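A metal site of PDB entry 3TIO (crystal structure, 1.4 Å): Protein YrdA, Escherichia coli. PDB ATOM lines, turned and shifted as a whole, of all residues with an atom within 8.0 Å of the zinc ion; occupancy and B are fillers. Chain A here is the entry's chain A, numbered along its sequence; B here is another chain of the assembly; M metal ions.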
ATOM      1  N   ARG A  45      34.529  -5.617 -16.611  1.00  0.00           N
ATOM      2  CA  ARG A  45      34.659  -7.040 -16.900  1.00  0.00           C
ATOM      3  C   ARG A  45      33.847  -7.456 -18.119  1.00  0.00           C
ATOM      4  O   ARG A  45      32.634  -7.426 -18.110  1.00  0.00           O
ATOM      5  CB  ARG A  45      34.237  -7.847 -15.655  1.00  0.00           C
ATOM      6  CG  ARG A  45      34.354  -9.365 -15.768  1.00  0.00           C
ATOM      7  CD  ARG A  45      34.709 -10.002 -14.422  1.00  0.00           C
ATOM      8  NE  ARG A  45      33.660  -9.911 -13.400  1.00  0.00           N
ATOM      9  CZ  ARG A  45      32.668 -10.788 -13.254  1.00  0.00           C
ATOM     10  NH1 ARG A  45      32.571 -11.829 -14.064  1.00  0.00           N
ATOM     11  NH2 ARG A  45      31.804 -10.645 -12.261  1.00  0.00           N
ATOM     12  N   ASP A  47      33.814 -10.580 -19.844  1.00  0.00           N
ATOM     13  CA  ASP A  47      34.140 -11.982 -20.007  1.00  0.00           C
ATOM     14  C   ASP A  47      33.153 -12.805 -20.826  1.00  0.00           C
ATOM     15  O   ASP A  47      33.530 -13.357 -21.860  1.00  0.00           O
ATOM     16  CB  ASP A  47      34.417 -12.651 -18.642  1.00  0.00           C
ATOM     17  CG  ASP A  47      33.473 -12.206 -17.538  1.00  0.00           C
ATOM     18  OD1 ASP A  47      33.752 -12.556 -16.375  1.00  0.00           O
ATOM     19  OD2 ASP A  47      32.459 -11.516 -17.808  1.00  0.00           O
ATOM     20  N   VAL A  48      31.898 -12.894 -20.392  1.00  0.00           N
ATOM     21  CA  VAL A  48      30.908 -13.673 -21.141  1.00  0.00           C
ATOM     22  C   VAL A  48      30.451 -12.945 -22.403  1.00  0.00           C
ATOM     23  O   VAL A  48      29.896 -13.563 -23.305  1.00  0.00           O
ATOM     24  CB  VAL A  48      29.680 -14.036 -20.274  1.00  0.00           C
ATOM     25  CG1 VAL A  48      30.086 -15.018 -19.193  1.00  0.00           C
ATOM     26  CG2 VAL A  48      29.078 -12.789 -19.664  1.00  0.00           C
ATOM     27  N   MET A  64      31.541   0.254 -11.668  1.00  0.00           N
ATOM     28  CA  MET A  64      31.615  -1.176 -11.897  1.00  0.00           C
ATOM     29  C   MET A  64      30.814  -1.436 -13.163  1.00  0.00           C
ATOM     30  O   MET A  64      29.607  -1.185 -13.204  1.00  0.00           O
ATOM     31  CB  MET A  64      31.013  -1.928 -10.703  1.00  0.00           C
ATOM     32  CG  MET A  64      31.492  -3.378 -10.524  1.00  0.00           C
ATOM     33  SD  MET A  64      30.865  -4.515 -11.777  1.00  0.00           S
ATOM     34  CE  MET A  64      32.363  -4.899 -12.696  1.00  0.00           C
ATOM     35  N   LEU A  65      31.499  -1.921 -14.193  1.00  0.00           N
ATOM     36  CA  LEU A  65      30.878  -2.202 -15.478  1.00  0.00           C
ATOM     37  C   LEU A  65      30.928  -3.678 -15.815  1.00  0.00           C
ATOM     38  O   LEU A  65      32.001  -4.276 -15.852  1.00  0.00           O
ATOM     39  CB  LEU A  65      31.599  -1.422 -16.588  1.00  0.00           C
ATOM     40  CG  LEU A  65      31.270   0.057 -16.789  1.00  0.00           C
ATOM     41  CD1 LEU A  65      31.484   0.838 -15.506  1.00  0.00           C
ATOM     42  CD2 LEU A  65      32.133   0.614 -17.913  1.00  0.00           C
ATOM     43  N   HIS A  66      29.763  -4.274 -16.049  1.00  0.00           N
ATOM     44  CA  HIS A  66      29.724  -5.676 -16.409  1.00  0.00           C
ATOM     45  C   HIS A  66      28.675  -5.901 -17.481  1.00  0.00           C
ATOM     46  O   HIS A  66      27.868  -5.021 -17.789  1.00  0.00           O
ATOM     47  CB  HIS A  66      29.414  -6.561 -15.190  1.00  0.00           C
ATOM     48  CG  HIS A  66      29.791  -7.997 -15.383  1.00  0.00           C
ATOM     49  ND1 HIS A  66      29.116  -9.030 -14.774  1.00  0.00           N
ATOM     50  CD2 HIS A  66      30.769  -8.567 -16.119  1.00  0.00           C
ATOM     51  CE1 HIS A  66      29.655 -10.182 -15.134  1.00  0.00           C
ATOM     52  NE2 HIS A  66      30.666  -9.934 -15.949  1.00  0.00           N
ATOM     53  N   VAL A  67      28.712  -7.103 -18.053  1.00  0.00           N
ATOM     54  CA  VAL A  67      27.800  -7.495 -19.117  1.00  0.00           C
ATOM     55  C   VAL A  67      26.681  -8.362 -18.570  1.00  0.00           C
ATOM     56  O   VAL A  67      26.737  -8.813 -17.426  1.00  0.00           O
ATOM     57  CB  VAL A  67      28.560  -8.286 -20.199  1.00  0.00           C
ATOM     58  CG1 VAL A  67      29.633  -7.401 -20.822  1.00  0.00           C
ATOM     59  CG2 VAL A  67      29.206  -9.515 -19.575  1.00  0.00           C
ATOM     60  N   THR A  68      25.660  -8.597 -19.388  1.00  0.00           N
ATOM     61  CA  THR A  68      24.552  -9.440 -18.976  1.00  0.00           C
ATOM     62  C   THR A  68      25.075 -10.869 -18.904  1.00  0.00           C
ATOM     63  O   THR A  68      25.755 -11.348 -19.803  1.00  0.00           O
ATOM     64  CB  THR A  68      23.388  -9.357 -19.986  1.00  0.00           C
ATOM     65  OG1 THR A  68      22.817  -8.048 -19.952  1.00  0.00           O
ATOM     66  CG2 THR A  68      22.319 -10.382 -19.661  1.00  0.00           C
ATOM     67  N   HIS A  69      24.759 -11.551 -17.803  1.00  0.00           N
ATOM     68  CA  HIS A  69      25.212 -12.917 -17.577  1.00  0.00           C
ATOM     69  C   HIS A  69      24.540 -13.920 -18.511  1.00  0.00           C
ATOM     70  O   HIS A  69      23.505 -13.634 -19.104  1.00  0.00           O
ATOM     71  CB  HIS A  69      24.938 -13.334 -16.132  1.00  0.00           C
ATOM     72  CG  HIS A  69      25.526 -12.419 -15.108  1.00  0.00           C
ATOM     73  ND1 HIS A  69      25.402 -12.640 -13.757  1.00  0.00           N
ATOM     74  CD2 HIS A  69      26.250 -11.284 -15.239  1.00  0.00           C
ATOM     75  CE1 HIS A  69      26.023 -11.675 -13.095  1.00  0.00           C
ATOM     76  NE2 HIS A  69      26.546 -10.840 -13.974  1.00  0.00           N
ATOM     77  N   MET A  93      27.066   1.896 -11.452  1.00  0.00           N
ATOM     78  CA  MET A  93      26.969   0.478 -11.748  1.00  0.00           C
ATOM     79  C   MET A  93      26.253   0.347 -13.087  1.00  0.00           C
ATOM     80  O   MET A  93      25.086   0.714 -13.199  1.00  0.00           O
ATOM     81  CB  MET A  93      26.133  -0.209 -10.653  1.00  0.00           C
ATOM     82  CG  MET A  93      25.795  -1.666 -10.891  1.00  0.00           C
ATOM     83  SD  MET A  93      27.060  -2.796 -10.311  1.00  0.00           S
ATOM     84  CE  MET A  93      27.528  -3.579 -11.876  1.00  0.00           C
ATOM     85  N   LEU A  94      26.965  -0.159 -14.104  1.00  0.00           N
ATOM     86  CA  LEU A  94      26.372  -0.349 -15.423  1.00  0.00           C
ATOM     87  C   LEU A  94      26.355  -1.848 -15.669  1.00  0.00           C
ATOM     88  O   LEU A  94      27.385  -2.513 -15.578  1.00  0.00           O
ATOM     89  CB  LEU A  94      27.181   0.349 -16.506  1.00  0.00           C
ATOM     90  CG  LEU A  94      27.354   1.859 -16.365  1.00  0.00           C
ATOM     91  CD1 LEU A  94      28.161   2.381 -17.539  1.00  0.00           C
ATOM     92  CD2 LEU A  94      25.997   2.549 -16.294  1.00  0.00           C
ATOM     93  N   HIS A  95      25.185  -2.375 -15.998  1.00  0.00           N
ATOM     94  CA  HIS A  95      25.076  -3.802 -16.199  1.00  0.00           C
ATOM     95  C   HIS A  95      24.310  -4.229 -17.446  1.00  0.00           C
ATOM     96  O   HIS A  95      23.084  -4.246 -17.447  1.00  0.00           O
ATOM     97  CB  HIS A  95      24.426  -4.429 -14.970  1.00  0.00           C
ATOM     98  CG  HIS A  95      24.839  -5.837 -14.728  1.00  0.00           C
ATOM     99  ND1 HIS A  95      24.158  -6.911 -15.242  1.00  0.00           N
ATOM    100  CD2 HIS A  95      25.928  -6.350 -14.095  1.00  0.00           C
ATOM    101  CE1 HIS A  95      24.803  -8.032 -14.940  1.00  0.00           C
ATOM    102  NE2 HIS A  95      25.872  -7.709 -14.248  1.00  0.00           N
ATOM    103  N   GLY A  96      25.057  -4.576 -18.493  1.00  0.00           N
ATOM    104  CA  GLY A  96      24.442  -5.026 -19.730  1.00  0.00           C
ATOM    105  C   GLY A  96      23.401  -4.116 -20.332  1.00  0.00           C
ATOM    106  O   GLY A  96      22.379  -4.582 -20.852  1.00  0.00           O
ATOM    107  N   ASP A 113      20.233  -4.478 -16.735  1.00  0.00           N
ATOM    108  CA  ASP A 113      20.216  -5.180 -18.008  1.00  0.00           C
ATOM    109  C   ASP A 113      19.089  -4.804 -18.951  1.00  0.00           C
ATOM    110  O   ASP A 113      17.930  -4.694 -18.556  1.00  0.00           O
ATOM    111  CB  ASP A 113      20.183  -6.686 -17.748  1.00  0.00           C
ATOM    112  CG  ASP A 113      21.317  -7.135 -16.864  1.00  0.00           C
ATOM    113  OD1 ASP A 113      22.284  -7.724 -17.380  1.00  0.00           O
ATOM    114  OD2 ASP A 113      21.229  -6.886 -15.643  1.00  0.00           O
ATOM    115  N   GLN B  60      30.403 -10.844  -5.563  1.00  0.00           N
ATOM    116  CA  GLN B  60      30.724 -10.128  -6.780  1.00  0.00           C
ATOM    117  C   GLN B  60      31.452  -8.799  -6.661  1.00  0.00           C
ATOM    118  O   GLN B  60      31.542  -8.215  -5.588  1.00  0.00           O
ATOM    119  CB  GLN B  60      29.462 -10.017  -7.625  1.00  0.00           C
ATOM    120  CG  GLN B  60      28.993 -11.408  -8.062  1.00  0.00           C
ATOM    121  CD  GLN B  60      27.706 -11.386  -8.843  1.00  0.00           C
ATOM    122  OE1 GLN B  60      27.613 -10.749  -9.891  1.00  0.00           O
ATOM    123  NE2 GLN B  60      26.697 -12.081  -8.338  1.00  0.00           N
ATOM    124  N   ASP B  61      31.974  -8.356  -7.806  1.00  0.00           N
ATOM    125  CA  ASP B  61      32.791  -7.142  -7.924  1.00  0.00           C
ATOM    126  C   ASP B  61      32.324  -5.933  -7.149  1.00  0.00           C
ATOM    127  O   ASP B  61      31.164  -5.554  -7.234  1.00  0.00           O
ATOM    128  CB  ASP B  61      32.938  -6.726  -9.397  1.00  0.00           C
ATOM    129  CG  ASP B  61      33.032  -7.893 -10.351  1.00  0.00           C
ATOM    130  OD1 ASP B  61      32.111  -8.750 -10.351  1.00  0.00           O
ATOM    131  OD2 ASP B  61      34.003  -7.954 -11.125  1.00  0.00           O
ATOM    132  N   GLY B  89      25.426  -9.935  -5.203  1.00  0.00           N
ATOM    133  CA  GLY B  89      25.610  -9.113  -6.390  1.00  0.00           C
ATOM    134  C   GLY B  89      26.696  -8.072  -6.338  1.00  0.00           C
ATOM    135  O   GLY B  89      27.261  -7.779  -5.290  1.00  0.00           O
ATOM    136  N   HIS B  90      26.986  -7.507  -7.507  1.00  0.00           N
ATOM    137  CA  HIS B  90      28.021  -6.472  -7.608  1.00  0.00           C
ATOM    138  C   HIS B  90      27.716  -5.322  -6.655  1.00  0.00           C
ATOM    139  O   HIS B  90      26.563  -4.959  -6.457  1.00  0.00           O
ATOM    140  CB  HIS B  90      28.082  -5.885  -9.012  1.00  0.00           C
ATOM    141  CG  HIS B  90      28.249  -6.895 -10.105  1.00  0.00           C
ATOM    142  ND1 HIS B  90      29.429  -7.559 -10.336  1.00  0.00           N
ATOM    143  CD2 HIS B  90      27.385  -7.311 -11.058  1.00  0.00           C
ATOM    144  CE1 HIS B  90      29.293  -8.344 -11.380  1.00  0.00           C
ATOM    145  NE2 HIS B  90      28.071  -8.209 -11.846  1.00  0.00           N
ATOM    146  N   MET B 107      22.385  -6.628  -6.961  1.00  0.00           N
ATOM    147  CA  MET B 107      23.486  -5.679  -7.029  1.00  0.00           C
ATOM    148  C   MET B 107      23.149  -4.297  -6.478  1.00  0.00           C
ATOM    149  O   MET B 107      22.051  -3.772  -6.682  1.00  0.00           O
ATOM    150  CB  MET B 107      24.015  -5.578  -8.474  1.00  0.00           C
ATOM    151  CG  MET B 107      23.073  -4.965  -9.481  1.00  0.00           C
ATOM    152  SD  MET B 107      23.756  -5.101 -11.157  1.00  0.00           S
ATOM    153  CE  MET B 107      22.848  -6.494 -11.797  1.00  0.00           C
ATOM    154  N   TYR B 167      28.062 -19.264 -11.249  1.00  0.00           N
ATOM    155  CA  TYR B 167      29.218 -18.526 -10.762  1.00  0.00           C
ATOM    156  C   TYR B 167      30.346 -19.449 -10.274  1.00  0.00           C
ATOM    157  O   TYR B 167      31.510 -19.048 -10.267  1.00  0.00           O
ATOM    158  CB  TYR B 167      28.808 -17.535  -9.664  1.00  0.00           C
ATOM    159  CG  TYR B 167      28.913 -16.099 -10.142  1.00  0.00           C
ATOM    160  CD1 TYR B 167      27.770 -15.340 -10.413  1.00  0.00           C
ATOM    161  CD2 TYR B 167      30.156 -15.517 -10.362  1.00  0.00           C
ATOM    162  CE1 TYR B 167      27.872 -14.041 -10.899  1.00  0.00           C
ATOM    163  CE2 TYR B 167      30.269 -14.211 -10.853  1.00  0.00           C
ATOM    164  CZ  TYR B 167      29.131 -13.482 -11.113  1.00  0.00           C
ATOM    165  OH  TYR B 167      29.241 -12.199 -11.582  1.00  0.00           O
ATOM    166  N   TRP B 170      32.018 -20.204 -13.289  1.00  0.00           N
ATOM    167  CA  TRP B 170      32.653 -18.960 -13.702  1.00  0.00           C
ATOM    168  C   TRP B 170      33.999 -18.773 -13.023  1.00  0.00           C
ATOM    169  O   TRP B 170      34.999 -18.471 -13.681  1.00  0.00           O
ATOM    170  CB  TRP B 170      31.733 -17.783 -13.369  1.00  0.00           C
ATOM    171  CG  TRP B 170      31.783 -16.640 -14.331  1.00  0.00           C
ATOM    172  CD1 TRP B 170      32.842 -16.257 -15.102  1.00  0.00           C
ATOM    173  CD2 TRP B 170      30.737 -15.698 -14.602  1.00  0.00           C
ATOM    174  NE1 TRP B 170      32.518 -15.141 -15.838  1.00  0.00           N
ATOM    175  CE2 TRP B 170      31.232 -14.775 -15.545  1.00  0.00           C
ATOM    176  CE3 TRP B 170      29.420 -15.547 -14.134  1.00  0.00           C
ATOM    177  CZ2 TRP B 170      30.470 -13.707 -16.032  1.00  0.00           C
ATOM    178  CZ3 TRP B 170      28.658 -14.478 -14.620  1.00  0.00           C
ATOM    179  CH2 TRP B 170      29.179 -13.581 -15.559  1.00  0.00           C
HETATM  180 ZN    ZN M   1      27.379  -8.963 -13.646  1.00  0.00          ZN
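OD1 of Asp 61 of chain B sits at hydrogen-bond distance from ND1 of His 90 of chain B, at 2.9 Å.
NE2 of His 95 lies close to O of Val 67 (3.5 Å).
NH1 of Arg 45 sits at hydrogen-bond distance from NE2 of His 66.
The side-chain amide oxygen (OE1) of Gln 60 of chain B lies close to a ring nitrogen (NE2) of His 90 of chain B.
The backbone NH of Asp 113 lies within hydrogen-bond range of the backbone carbonyl oxygen of His 95 (2.9 Å).
A ring nitrogen (NE2) of His 66 lies within hydrogen-bond range of the side-chain carboxylate of Asp 47.
The backbone carbonyl oxygen (O) of His 66 sits at hydrogen-bond distance from the backbone NH (N) of Gly 96 (2.9 Å).
A ring nitrogen (ND1) of His 90 of chain B is in hydrogen-bond range of the side-chain sulfur (SD) of Met 64 (3.7 Å).
The zinc ion is bound by NE2 of His 95 (2.1 Å), NE2 of His 90 of chain B (2.1 Å), ND1 of His 66 (2.1 Å) and NE2 of His 69 (2.1 Å).
The zinc ion has four donor atoms within binding distance.
Residues that only touch the zinc ion: Val 67 (3.8 Å).
Of the 21 residues printed, 5 come within 4 Å of the zinc ion.
Along chain A the residues within 4 Å of the zinc ion span positions 66 to 95.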
